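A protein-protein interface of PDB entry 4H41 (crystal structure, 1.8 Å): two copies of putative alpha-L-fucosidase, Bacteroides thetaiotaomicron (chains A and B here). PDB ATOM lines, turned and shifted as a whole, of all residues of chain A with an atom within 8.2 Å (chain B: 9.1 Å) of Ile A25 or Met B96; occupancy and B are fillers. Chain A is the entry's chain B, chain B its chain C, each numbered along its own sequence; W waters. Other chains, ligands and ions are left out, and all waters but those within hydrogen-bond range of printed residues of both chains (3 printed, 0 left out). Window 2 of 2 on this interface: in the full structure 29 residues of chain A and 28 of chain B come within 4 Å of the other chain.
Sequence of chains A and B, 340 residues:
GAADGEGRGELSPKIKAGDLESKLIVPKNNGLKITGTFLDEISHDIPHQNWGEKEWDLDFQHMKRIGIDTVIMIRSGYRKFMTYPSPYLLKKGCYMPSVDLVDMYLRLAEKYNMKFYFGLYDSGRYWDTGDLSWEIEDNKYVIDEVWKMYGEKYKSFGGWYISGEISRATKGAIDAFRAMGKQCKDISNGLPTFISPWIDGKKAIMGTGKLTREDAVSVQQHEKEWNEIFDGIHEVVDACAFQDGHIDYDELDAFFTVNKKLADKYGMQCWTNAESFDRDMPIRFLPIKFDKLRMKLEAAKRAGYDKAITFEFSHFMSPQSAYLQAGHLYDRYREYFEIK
The backbone NH (N) of Asp B103 is in hydrogen-bond range of the side-chain carboxylate (OD1) of Asp B100, 3.0 Å away. The backbone NH (N) of Tyr B95 lies within hydrogen-bond range of the backbone carbonyl oxygen (O) of Lys B80, at 2.8 Å. The guanidinium group (NH1) of Arg A294 is in salt-bridge range of the side-chain carboxylate (OE2) of Glu A298. OH of Tyr B150 is in hydrogen-bond range of OD2 of Asp B100 (2.7 Å). The guanidinium group of Arg A294 lies within salt-bridge range of the side-chain carboxylate of Asp A291 (3.0 Å). The backbone NH of Val B102 lies within hydrogen-bond range of the side-chain carboxylate of Asp B100 (3.2 Å).
Ser A22 touches Val B99 (CB to CG2, 3.4 Å). Ser B98 touches Leu A24. Val B99 touches Leu A24 (CG2 to CD2, 3.8 Å). CG1 of Ile A25 touches O of Pro B97, at 3.2 Å. Asp B100 touches Ile A25 (N to CD1, 3.9 Å). Met B96 touches Val A26. CG1 of Val A26 touches O of Pro B97, 3.5 Å away. Ser B98 touches Val A26. NH2 of Arg A294 touches C of Pro B97 (3.98 Å). NH2 of Arg A294 touches N of Ser B98, at 3.6 Å.
No position is printed for both chains.
O of Ser B98 is in hydrogen-bond range of N of Ile A25 (2.9 Å). The side-chain hydroxyl (OG) of Ser B98 sits at hydrogen-bond distance from the side-chain carboxylate (OD1) of Asp A291 (2.7 Å). The backbone carbonyl oxygen (O) of Met B96 lies within hydrogen-bond range of the guanidinium group (NH2) of Arg A294, 3.3 Å away.
Printed residues of chain A that touch a printed residue of chain B: Ser A22, Lys A23, Leu A24, Ile A25, Val A26, Asp A291, Arg A294 and Met A295. Printed residues of chain B that touch a printed residue of chain A: Phe B81, Tyr B95, Met B96, Pro B97, Ser B98, Val B99 and Asp B100. Hydrophobic or aromatic side chains of chain B within 4 Å of the printed part of chain A: Phe B81, Tyr B95, Met B96, Pro B97 and Val B99. Among the printed residues, 18 pairs touch across the chains. Among the printed residues, no Asp or Glu carboxylate lies within 4 Å of a Lys or Arg side-chain nitrogen of the other chain.
Ile A25 touches just these residues of chain B: Met B96, Pro B97, Ser B98 and Asp B100. Val A26 touches just these residues of chain B: Met B96 (3.6 Å), Pro B97 (3.5 Å) and Ser B98 (3.9 Å). Of chain A, only Ile A25 (3.2 Å), Val A26 (3.5 Å), Asp A291 (3.6 Å) and Arg A294 (3.98 Å) come within 4 Å of Pro B97. Of the printed residues of chain A, Phe B81 touches Met A295 (3.5 Å). Printed residues of chain A within 4 Å of Ser B98: Lys A23 (3.7 Å), Leu A24 (3.1 Å), Ile A25 (2.9 Å), Val A26 (3.9 Å), Asp A291 (2.7 Å) and Arg A294 (3.6 Å). Of the printed residues of chain A, Tyr B95 touches Met A295 (3.7 Å). Of the printed residues of chain B, Asp A291 touches Pro B97 (3.6 Å) and Ser B98 (2.7 Å). The nearest printed residue of chain B that does not touch Ile A25 is Val B99 (4.04 Å). The nearest residue of chain A that does not touch Met B96 is Asp A291 (5.0 Å). The nearest printed residue of chain B that does not touch Met A295 is Met B96 (5.6 Å).
Water W3 lies within hydrogen-bond range of O of Lys A23 (2.6 Å) and N of Asp B100 (2.9 Å). Water W2 lies within hydrogen-bond range of O of Met B96 (2.6 Å) and NH1 of Arg A294 (3.5 Å). Water W1 lies within hydrogen-bond range of the guanidinium group (NH2) of Arg A294 (2.8 Å), the backbone carbonyl oxygen (O) of Met B96 (2.9 Å) and the side-chain sulfur (SD) of Met A295 (3.4 Å).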
ATOM      1  N   SER A  22      37.420 -15.063 -27.373  1.00  0.00           N
ATOM      2  CA  SER A  22      36.179 -14.284 -27.426  1.00  0.00           C
ATOM      3  C   SER A  22      36.334 -13.106 -26.475  1.00  0.00           C
ATOM      4  O   SER A  22      37.050 -13.185 -25.469  1.00  0.00           O
ATOM      5  CB  SER A  22      34.985 -15.136 -26.989  1.00  0.00           C
ATOM      6  OG  SER A  22      34.898 -16.407 -27.654  1.00  0.00           O
ATOM      7  N   LYS A  23      35.671 -12.023 -26.773  1.00  0.00           N
ATOM      8  CA  LYS A  23      35.703 -10.849 -25.920  1.00  0.00           C
ATOM      9  C   LYS A  23      34.659 -11.084 -24.861  1.00  0.00           C
ATOM     10  O   LYS A  23      33.496 -11.167 -25.227  1.00  0.00           O
ATOM     11  CB  LYS A  23      35.419  -9.600 -26.779  1.00  0.00           C
ATOM     12  CG  LYS A  23      35.654  -8.244 -26.084  1.00  0.00           C
ATOM     13  CD  LYS A  23      34.508  -7.805 -25.180  1.00  0.00           C
ATOM     14  CE  LYS A  23      34.269  -6.307 -25.111  1.00  0.00           C
ATOM     15  NZ  LYS A  23      32.975  -5.879 -25.742  1.00  0.00           N
ATOM     16  N   LEU A  24      35.048 -11.275 -23.552  1.00  0.00           N
ATOM     17  CA  LEU A  24      34.011 -11.522 -22.540  1.00  0.00           C
ATOM     18  C   LEU A  24      33.297 -10.220 -22.185  1.00  0.00           C
ATOM     19  O   LEU A  24      33.925  -9.183 -22.022  1.00  0.00           O
ATOM     20  CB  LEU A  24      34.537 -12.200 -21.270  1.00  0.00           C
ATOM     21  CG  LEU A  24      35.146 -13.599 -21.413  1.00  0.00           C
ATOM     22  CD1 LEU A  24      35.099 -14.311 -20.076  1.00  0.00           C
ATOM     23  CD2 LEU A  24      34.443 -14.460 -22.467  1.00  0.00           C
ATOM     24  N   ILE A  25      31.990 -10.277 -22.038  1.00  0.00           N
ATOM     25  CA  ILE A  25      31.182  -9.116 -21.707  1.00  0.00           C
ATOM     26  C   ILE A  25      30.591  -9.251 -20.306  1.00  0.00           C
ATOM     27  O   ILE A  25      29.723  -8.484 -19.927  1.00  0.00           O
ATOM     28  CB  ILE A  25      30.099  -8.831 -22.780  1.00  0.00           C
ATOM     29  CG1 ILE A  25      29.127 -10.026 -22.966  1.00  0.00           C
ATOM     30  CG2 ILE A  25      30.770  -8.453 -24.100  1.00  0.00           C
ATOM     31  CD1 ILE A  25      27.995  -9.764 -23.868  1.00  0.00           C
ATOM     32  N   VAL A  26      31.129 -10.173 -19.511  1.00  0.00           N
ATOM     33  CA  VAL A  26      30.782 -10.320 -18.110  1.00  0.00           C
ATOM     34  C   VAL A  26      32.076 -10.215 -17.309  1.00  0.00           C
ATOM     35  O   VAL A  26      33.154 -10.551 -17.819  1.00  0.00           O
ATOM     36  CB  VAL A  26      30.023 -11.648 -17.774  1.00  0.00           C
ATOM     37  CG1 VAL A  26      28.676 -11.707 -18.480  1.00  0.00           C
ATOM     38  CG2 VAL A  26      30.845 -12.880 -18.051  1.00  0.00           C
ATOM     39  N   PRO A  27      31.978  -9.875 -16.012  1.00  0.00           N
ATOM     40  CA  PRO A  27      33.199  -9.867 -15.178  1.00  0.00           C
ATOM     41  C   PRO A  27      33.847 -11.255 -15.076  1.00  0.00           C
ATOM     42  O   PRO A  27      33.168 -12.281 -14.952  1.00  0.00           O
ATOM     43  CB  PRO A  27      32.700  -9.373 -13.811  1.00  0.00           C
ATOM     44  CG  PRO A  27      31.446  -8.625 -14.115  1.00  0.00           C
ATOM     45  CD  PRO A  27      30.813  -9.393 -15.249  1.00  0.00           C
ATOM     46  N   LYS A  28      35.167 -11.283 -15.157  1.00  0.00           N
ATOM     47  CA  LYS A  28      35.919 -12.533 -15.072  1.00  0.00           C
ATOM     48  C   LYS A  28      36.139 -12.933 -13.600  1.00  0.00           C
ATOM     49  O   LYS A  28      35.985 -12.116 -12.691  1.00  0.00           O
ATOM     50  CB  LYS A  28      37.246 -12.417 -15.814  1.00  0.00           C
ATOM     51  CG  LYS A  28      38.246 -11.488 -15.105  1.00  0.00           C
ATOM     52  CD  LYS A  28      39.321 -10.958 -16.014  1.00  0.00           C
ATOM     53  CE  LYS A  28      40.264 -10.070 -15.218  1.00  0.00           C
ATOM     54  NZ  LYS A  28      41.438  -9.628 -16.015  1.00  0.00           N
ATOM     55  N   ASP A 291      28.463 -21.295 -20.260  1.00  0.00           N
ATOM     56  CA  ASP A 291      27.697 -20.209 -19.590  1.00  0.00           C
ATOM     57  C   ASP A 291      26.755 -20.728 -18.540  1.00  0.00           C
ATOM     58  O   ASP A 291      26.563 -20.068 -17.532  1.00  0.00           O
ATOM     59  CB  ASP A 291      26.930 -19.313 -20.574  1.00  0.00           C
ATOM     60  CG  ASP A 291      27.747 -18.140 -21.103  1.00  0.00           C
ATOM     61  OD1 ASP A 291      28.841 -17.868 -20.543  1.00  0.00           O
ATOM     62  OD2 ASP A 291      27.234 -17.415 -21.990  1.00  0.00           O
ATOM     63  N   ARG A 294      29.056 -21.474 -15.609  1.00  0.00           N
ATOM     64  CA  ARG A 294      29.506 -20.156 -15.104  1.00  0.00           C
ATOM     65  C   ARG A 294      28.414 -19.583 -14.201  1.00  0.00           C
ATOM     66  O   ARG A 294      28.700 -19.080 -13.149  1.00  0.00           O
ATOM     67  CB  ARG A 294      29.816 -19.191 -16.272  1.00  0.00           C
ATOM     68  CG  ARG A 294      30.253 -17.880 -15.789  1.00  0.00           C
ATOM     69  CD  ARG A 294      30.474 -16.852 -16.855  1.00  0.00           C
ATOM     70  NE  ARG A 294      29.397 -16.745 -17.813  1.00  0.00           N
ATOM     71  CZ  ARG A 294      28.260 -16.073 -17.666  1.00  0.00           C
ATOM     72  NH1 ARG A 294      28.021 -15.386 -16.557  1.00  0.00           N
ATOM     73  NH2 ARG A 294      27.380 -16.034 -18.647  1.00  0.00           N
ATOM     74  N   MET A 295      27.177 -19.594 -14.659  1.00  0.00           N
ATOM     75  CA  MET A 295      26.081 -19.025 -13.851  1.00  0.00           C
ATOM     76  C   MET A 295      25.920 -19.767 -12.509  1.00  0.00           C
ATOM     77  O   MET A 295      25.650 -19.128 -11.493  1.00  0.00           O
ATOM     78  CB  MET A 295      24.786 -19.055 -14.648  1.00  0.00           C
ATOM     79  CG  MET A 295      24.754 -18.029 -15.736  1.00  0.00           C
ATOM     80  SD  MET A 295      22.957 -18.140 -16.603  1.00  0.00           S
ATOM     81  CE  MET A 295      22.603 -19.983 -16.872  1.00  0.00           C
ATOM     82  N   GLU A 298      28.812 -18.698 -10.301  1.00  0.00           N
ATOM     83  CA  GLU A 298      28.583 -17.307  -9.910  1.00  0.00           C
ATOM     84  C   GLU A 298      27.567 -17.247  -8.753  1.00  0.00           C
ATOM     85  O   GLU A 298      27.745 -16.479  -7.824  1.00  0.00           O
ATOM     86  CB  GLU A 298      28.119 -16.447 -11.090  1.00  0.00           C
ATOM     87  CG  GLU A 298      29.252 -16.176 -12.055  1.00  0.00           C
ATOM     88  CD  GLU A 298      28.879 -15.443 -13.327  1.00  0.00           C
ATOM     89  OE1 GLU A 298      27.671 -15.182 -13.549  1.00  0.00           O
ATOM     90  OE2 GLU A 298      29.804 -15.157 -14.125  1.00  0.00           O
ATOM     91  N   LYS B  80      15.227 -17.637 -21.395  1.00  0.00           N
ATOM     92  CA  LYS B  80      16.088 -16.634 -20.735  1.00  0.00           C
ATOM     93  C   LYS B  80      17.523 -16.576 -21.273  1.00  0.00           C
ATOM     94  O   LYS B  80      18.296 -15.736 -20.827  1.00  0.00           O
ATOM     95  CB  LYS B  80      16.090 -16.857 -19.236  1.00  0.00           C
ATOM     96  CG  LYS B  80      14.708 -16.522 -18.645  1.00  0.00           C
ATOM     97  CD  LYS B  80      14.702 -16.482 -17.128  1.00  0.00           C
ATOM     98  CE  LYS B  80      13.452 -15.823 -16.611  1.00  0.00           C
ATOM     99  NZ  LYS B  80      13.439 -15.723 -15.134  1.00  0.00           N
ATOM    100  N   PHE B  81      17.861 -17.401 -22.231  1.00  0.00           N
ATOM    101  CA  PHE B  81      19.200 -17.378 -22.856  1.00  0.00           C
ATOM    102  C   PHE B  81      19.186 -16.471 -24.089  1.00  0.00           C
ATOM    103  O   PHE B  81      18.200 -16.439 -24.833  1.00  0.00           O
ATOM    104  CB  PHE B  81      19.659 -18.790 -23.212  1.00  0.00           C
ATOM    105  CG  PHE B  81      20.042 -19.583 -21.992  1.00  0.00           C
ATOM    106  CD1 PHE B  81      21.297 -19.456 -21.435  1.00  0.00           C
ATOM    107  CD2 PHE B  81      19.102 -20.342 -21.322  1.00  0.00           C
ATOM    108  CE1 PHE B  81      21.615 -20.097 -20.241  1.00  0.00           C
ATOM    109  CE2 PHE B  81      19.443 -21.054 -20.176  1.00  0.00           C
ATOM    110  CZ  PHE B  81      20.664 -20.864 -19.594  1.00  0.00           C
ATOM    111  N   MET B  82      20.278 -15.722 -24.296  1.00  0.00           N
ATOM    112  CA  MET B  82      20.400 -14.819 -25.427  1.00  0.00           C
ATOM    113  C   MET B  82      21.812 -14.893 -26.022  1.00  0.00           C
ATOM    114  O   MET B  82      22.760 -15.341 -25.387  1.00  0.00           O
ATOM    115  CB  MET B  82      20.047 -13.372 -25.047  1.00  0.00           C
ATOM    116  CG  MET B  82      21.003 -12.769 -24.062  1.00  0.00           C
ATOM    117  SD  MET B  82      20.411 -10.984 -23.477  1.00  0.00           S
ATOM    118  CE  MET B  82      19.231 -11.465 -22.122  1.00  0.00           C
ATOM    119  N   THR B  83      21.925 -14.415 -27.249  1.00  0.00           N
ATOM    120  CA  THR B  83      23.168 -14.444 -28.036  1.00  0.00           C
ATOM    121  C   THR B  83      23.902 -13.129 -28.069  1.00  0.00           C
ATOM    122  O   THR B  83      24.989 -13.059 -28.649  1.00  0.00           O
ATOM    123  CB  THR B  83      22.847 -14.855 -29.473  1.00  0.00           C
ATOM    124  OG1 THR B  83      22.005 -13.864 -30.079  1.00  0.00           O
ATOM    125  CG2 THR B  83      22.232 -16.240 -29.555  1.00  0.00           C
ATOM    126  N   TYR B  84      23.316 -12.085 -27.510  1.00  0.00           N
ATOM    127  CA  TYR B  84      23.900 -10.745 -27.542  1.00  0.00           C
ATOM    128  C   TYR B  84      23.381  -9.957 -26.353  1.00  0.00           C
ATOM    129  O   TYR B  84      22.348 -10.348 -25.774  1.00  0.00           O
ATOM    130  CB  TYR B  84      23.548 -10.071 -28.891  1.00  0.00           C
ATOM    131  CG  TYR B  84      22.113  -9.588 -29.023  1.00  0.00           C
ATOM    132  CD1 TYR B  84      21.092 -10.458 -29.384  1.00  0.00           C
ATOM    133  CD2 TYR B  84      21.781  -8.252 -28.801  1.00  0.00           C
ATOM    134  CE1 TYR B  84      19.773 -10.036 -29.446  1.00  0.00           C
ATOM    135  CE2 TYR B  84      20.472  -7.802 -28.943  1.00  0.00           C
ATOM    136  CZ  TYR B  84      19.469  -8.698 -29.265  1.00  0.00           C
ATOM    137  OH  TYR B  84      18.156  -8.309 -29.322  1.00  0.00           O
ATOM    138  N   PRO B  85      24.031  -8.828 -25.981  1.00  0.00           N
ATOM    139  CA  PRO B  85      23.585  -8.086 -24.785  1.00  0.00           C
ATOM    140  C   PRO B  85      22.383  -7.211 -25.092  1.00  0.00           C
ATOM    141  O   PRO B  85      22.504  -6.012 -25.256  1.00  0.00           O
ATOM    142  CB  PRO B  85      24.830  -7.292 -24.385  1.00  0.00           C
ATOM    143  CG  PRO B  85      25.539  -7.064 -25.659  1.00  0.00           C
ATOM    144  CD  PRO B  85      25.284  -8.260 -26.526  1.00  0.00           C
ATOM    145  N   SER B  86      21.233  -7.826 -25.173  1.00  0.00           N
ATOM    146  CA  SER B  86      19.983  -7.126 -25.472  1.00  0.00           C
ATOM    147  C   SER B  86      19.516  -6.236 -24.330  1.00  0.00           C
ATOM    148  O   SER B  86      19.092  -6.769 -23.301  1.00  0.00           O
ATOM    149  CB  SER B  86      18.882  -8.145 -25.764  1.00  0.00           C
ATOM    150  OG  SER B  86      17.605  -7.556 -25.944  1.00  0.00           O
ATOM    151  N   PRO B  87      19.445  -4.899 -24.506  1.00  0.00           N
ATOM    152  CA  PRO B  87      18.875  -4.062 -23.418  1.00  0.00           C
ATOM    153  C   PRO B  87      17.434  -4.471 -23.082  1.00  0.00           C
ATOM    154  O   PRO B  87      17.092  -4.576 -21.920  1.00  0.00           O
ATOM    155  CB  PRO B  87      18.956  -2.642 -23.973  1.00  0.00           C
ATOM    156  CG  PRO B  87      20.010  -2.689 -24.998  1.00  0.00           C
ATOM    157  CD  PRO B  87      19.938  -4.061 -25.614  1.00  0.00           C
ATOM    158  N   LEU B  89      15.805  -7.610 -23.573  1.00  0.00           N
ATOM    159  CA  LEU B  89      15.706  -8.914 -22.925  1.00  0.00           C
ATOM    160  C   LEU B  89      16.331  -8.894 -21.526  1.00  0.00           C
ATOM    161  O   LEU B  89      15.806  -9.541 -20.636  1.00  0.00           O
ATOM    162  CB  LEU B  89      16.339 -10.019 -23.780  1.00  0.00           C
ATOM    163  CG  LEU B  89      15.664 -10.284 -25.137  1.00  0.00           C
ATOM    164  CD1 LEU B  89      16.450 -11.275 -25.938  1.00  0.00           C
ATOM    165  CD2 LEU B  89      14.224 -10.793 -24.950  1.00  0.00           C
ATOM    166  N   LEU B  90      17.375  -8.097 -21.316  1.00  0.00           N
ATOM    167  CA  LEU B  90      17.968  -7.958 -19.981  1.00  0.00           C
ATOM    168  C   LEU B  90      16.951  -7.329 -19.023  1.00  0.00           C
ATOM    169  O   LEU B  90      16.827  -7.783 -17.895  1.00  0.00           O
ATOM    170  CB  LEU B  90      19.254  -7.138 -20.031  1.00  0.00           C
ATOM    171  CG  LEU B  90      20.439  -7.871 -20.648  1.00  0.00           C
ATOM    172  CD1 LEU B  90      21.550  -6.900 -21.027  1.00  0.00           C
ATOM    173  CD2 LEU B  90      20.972  -8.962 -19.681  1.00  0.00           C
ATOM    174  N   LYS B  91      16.179  -6.342 -19.482  1.00  0.00           N
ATOM    175  CA  LYS B  91      15.142  -5.721 -18.643  1.00  0.00           C
ATOM    176  C   LYS B  91      14.025  -6.689 -18.320  1.00  0.00           C
ATOM    177  O   LYS B  91      13.401  -6.551 -17.282  1.00  0.00           O
ATOM    178  CB  LYS B  91      14.544  -4.456 -19.307  1.00  0.00           C
ATOM    179  CG  LYS B  91      15.479  -3.265 -19.314  1.00  0.00           C
ATOM    180  CD  LYS B  91      14.894  -2.057 -20.092  1.00  0.00           C
ATOM    181  CE  LYS B  91      15.774  -1.623 -21.250  1.00  0.00           C
ATOM    182  NZ  LYS B  91      15.360  -0.328 -21.849  1.00  0.00           N
ATOM    183  N   GLY B  93      14.511  -9.803 -17.547  1.00  0.00           N
ATOM    184  CA  GLY B  93      15.053 -10.827 -16.659  1.00  0.00           C
ATOM    185  C   GLY B  93      15.825 -11.955 -17.326  1.00  0.00           C
ATOM    186  O   GLY B  93      16.107 -12.970 -16.681  1.00  0.00           O
ATOM    187  N   CYS B  94      16.242 -11.779 -18.580  1.00  0.00           N
ATOM    188  CA  CYS B  94      17.017 -12.808 -19.261  1.00  0.00           C
ATOM    189  C   CYS B  94      18.508 -12.693 -18.878  1.00  0.00           C
ATOM    190  O   CYS B  94      18.936 -11.697 -18.297  1.00  0.00           O
ATOM    191  CB  CYS B  94      16.801 -12.715 -20.755  1.00  0.00           C
ATOM    192  SG  CYS B  94      15.076 -12.942 -21.255  1.00  0.00           S
ATOM    193  N   TYR B  95      19.264 -13.747 -19.128  1.00  0.00           N
ATOM    194  CA  TYR B  95      20.646 -13.877 -18.650  1.00  0.00           C
ATOM    195  C   TYR B  95      21.669 -13.236 -19.562  1.00  0.00           C
ATOM    196  O   TYR B  95      21.713 -13.520 -20.743  1.00  0.00           O
ATOM    197  CB  TYR B  95      21.004 -15.355 -18.525  1.00  0.00           C
ATOM    198  CG  TYR B  95      20.010 -16.217 -17.764  1.00  0.00           C
ATOM    199  CD1 TYR B  95      19.347 -15.730 -16.636  1.00  0.00           C
ATOM    200  CD2 TYR B  95      19.709 -17.503 -18.193  1.00  0.00           C
ATOM    201  CE1 TYR B  95      18.437 -16.516 -15.946  1.00  0.00           C
ATOM    202  CE2 TYR B  95      18.776 -18.284 -17.533  1.00  0.00           C
ATOM    203  CZ  TYR B  95      18.126 -17.782 -16.418  1.00  0.00           C
ATOM    204  OH  TYR B  95      17.242 -18.553 -15.719  1.00  0.00           O
ATOM    205  N   MET B  96      22.559 -12.426 -18.987  1.00  0.00           N
ATOM    206  CA  MET B  96      23.647 -11.850 -19.756  1.00  0.00           C
ATOM    207  C   MET B  96      24.568 -12.997 -20.248  1.00  0.00           C
ATOM    208  O   MET B  96      25.040 -13.778 -19.434  1.00  0.00           O
ATOM    209  CB  MET B  96      24.441 -10.861 -18.867  1.00  0.00           C
ATOM    210  CG  MET B  96      25.601 -10.186 -19.552  1.00  0.00           C
ATOM    211  SD  MET B  96      24.987  -8.847 -20.864  1.00  0.00           S
ATOM    212  CE  MET B  96      26.686  -7.807 -20.929  1.00  0.00           C
ATOM    213  N   PRO B  97      24.833 -13.114 -21.551  1.00  0.00           N
ATOM    214  CA  PRO B  97      25.792 -14.126 -22.016  1.00  0.00           C
ATOM    215  C   PRO B  97      27.215 -13.646 -21.822  1.00  0.00           C
ATOM    216  O   PRO B  97      27.437 -12.436 -21.682  1.00  0.00           O
ATOM    217  CB  PRO B  97      25.461 -14.251 -23.500  1.00  0.00           C
ATOM    218  CG  PRO B  97      25.018 -12.882 -23.867  1.00  0.00           C
ATOM    219  CD  PRO B  97      24.360 -12.278 -22.679  1.00  0.00           C
ATOM    220  N   SER B  98      28.198 -14.555 -21.873  1.00  0.00           N
ATOM    221  CA  SER B  98      29.573 -14.093 -21.667  1.00  0.00           C
ATOM    222  C   SER B  98      30.190 -13.564 -22.944  1.00  0.00           C
ATOM    223  O   SER B  98      31.225 -12.916 -22.841  1.00  0.00           O
ATOM    224  CB  SER B  98      30.448 -15.200 -21.098  1.00  0.00           C
ATOM    225  OG  SER B  98      30.491 -16.321 -21.959  1.00  0.00           O
ATOM    226  N   VAL B  99      29.615 -13.865 -24.120  1.00  0.00           N
ATOM    227  CA  VAL B  99      30.142 -13.427 -25.405  1.00  0.00           C
ATOM    228  C   VAL B  99      29.018 -12.860 -26.251  1.00  0.00           C
ATOM    229  O   VAL B  99      27.952 -13.455 -26.329  1.00  0.00           O
ATOM    230  CB  VAL B  99      30.845 -14.607 -26.163  1.00  0.00           C
ATOM    231  CG1 VAL B  99      31.320 -14.182 -27.563  1.00  0.00           C
ATOM    232  CG2 VAL B  99      32.007 -15.185 -25.348  1.00  0.00           C
ATOM    233  N   ASP B 100      29.296 -11.765 -26.961  1.00  0.00           N
ATOM    234  CA  ASP B 100      28.357 -11.221 -27.952  1.00  0.00           C
ATOM    235  C   ASP B 100      28.543 -12.043 -29.243  1.00  0.00           C
ATOM    236  O   ASP B 100      29.445 -11.766 -30.053  1.00  0.00           O
ATOM    237  CB  ASP B 100      28.581  -9.724 -28.188  1.00  0.00           C
ATOM    238  CG  ASP B 100      27.581  -9.108 -29.154  1.00  0.00           C
ATOM    239  OD1 ASP B 100      26.889  -9.871 -29.855  1.00  0.00           O
ATOM    240  OD2 ASP B 100      27.548  -7.857 -29.250  1.00  0.00           O
ATOM    241  N   LEU B 101      27.717 -13.073 -29.410  1.00  0.00           N
ATOM    242  CA  LEU B 101      27.795 -13.963 -30.587  1.00  0.00           C
ATOM    243  C   LEU B 101      27.355 -13.280 -31.852  1.00  0.00           C
ATOM    244  O   LEU B 101      27.867 -13.601 -32.917  1.00  0.00           O
ATOM    245  CB  LEU B 101      26.953 -15.228 -30.385  1.00  0.00           C
ATOM    246  CG  LEU B 101      27.372 -16.114 -29.215  1.00  0.00           C
ATOM    247  CD1 LEU B 101      26.373 -17.288 -29.037  1.00  0.00           C
ATOM    248  CD2 LEU B 101      28.762 -16.663 -29.415  1.00  0.00           C
ATOM    249  N   VAL B 102      26.417 -12.357 -31.770  1.00  0.00           N
ATOM    250  CA  VAL B 102      25.936 -11.622 -32.961  1.00  0.00           C
ATOM    251  C   VAL B 102      27.117 -10.837 -33.568  1.00  0.00           C
ATOM    252  O   VAL B 102      27.383 -10.945 -34.770  1.00  0.00           O
ATOM    253  CB  VAL B 102      24.721 -10.739 -32.651  1.00  0.00           C
ATOM    254  CG1 VAL B 102      24.323  -9.930 -33.868  1.00  0.00           C
ATOM    255  CG2 VAL B 102      23.536 -11.602 -32.215  1.00  0.00           C
ATOM    256  N   ASP B 103      27.830 -10.084 -32.734  1.00  0.00           N
ATOM    257  CA  ASP B 103      29.025  -9.342 -33.138  1.00  0.00           C
ATOM    258  C   ASP B 103      30.042 -10.297 -33.758  1.00  0.00           C
ATOM    259  O   ASP B 103      30.579 -10.017 -34.834  1.00  0.00           O
ATOM    260  CB  ASP B 103      29.654  -8.630 -31.928  1.00  0.00           C
ATOM    261  CG  ASP B 103      31.072  -8.134 -32.189  1.00  0.00           C
ATOM    262  OD1 ASP B 103      31.219  -7.187 -32.940  1.00  0.00           O
ATOM    263  OD2 ASP B 103      32.037  -8.785 -31.704  1.00  0.00           O
ATOM    264  N   MET B 149      21.735  -1.616 -33.460  1.00  0.00           N
ATOM    265  CA  MET B 149      22.991  -2.056 -32.865  1.00  0.00           C
ATOM    266  C   MET B 149      23.905  -2.767 -33.859  1.00  0.00           C
ATOM    267  O   MET B 149      25.124  -2.615 -33.777  1.00  0.00           O
ATOM    268  CB  MET B 149      22.717  -2.995 -31.679  1.00  0.00           C
ATOM    269  CG  MET B 149      22.073  -2.317 -30.479  1.00  0.00           C
ATOM    270  SD  MET B 149      21.421  -3.719 -29.216  1.00  0.00           S
ATOM    271  CE  MET B 149      23.161  -4.283 -28.550  1.00  0.00           C
ATOM    272  N   TYR B 150      23.328  -3.544 -34.792  1.00  0.00           N
ATOM    273  CA  TYR B 150      24.084  -4.399 -35.716  1.00  0.00           C
ATOM    274  C   TYR B 150      23.765  -4.142 -37.194  1.00  0.00           C
ATOM    275  O   TYR B 150      24.678  -3.994 -37.993  1.00  0.00           O
ATOM    276  CB  TYR B 150      23.790  -5.870 -35.421  1.00  0.00           C
ATOM    277  CG  TYR B 150      24.133  -6.269 -34.004  1.00  0.00           C
ATOM    278  CD1 TYR B 150      25.453  -6.400 -33.598  1.00  0.00           C
ATOM    279  CD2 TYR B 150      23.141  -6.409 -33.041  1.00  0.00           C
ATOM    280  CE1 TYR B 150      25.779  -6.734 -32.288  1.00  0.00           C
ATOM    281  CE2 TYR B 150      23.459  -6.693 -31.718  1.00  0.00           C
ATOM    282  CZ  TYR B 150      24.781  -6.854 -31.344  1.00  0.00           C
ATOM    283  OH  TYR B 150      25.093  -7.091 -30.031  1.00  0.00           O
HETATM  284  O   HOH W   1      24.668 -16.622 -19.078  1.00  0.00           O
HETATM  285  O   HOH W   2      24.838 -14.084 -16.856  1.00  0.00           O
HETATM  286  O   HOH W   3      31.871 -10.368 -27.072  1.00  0.00           O
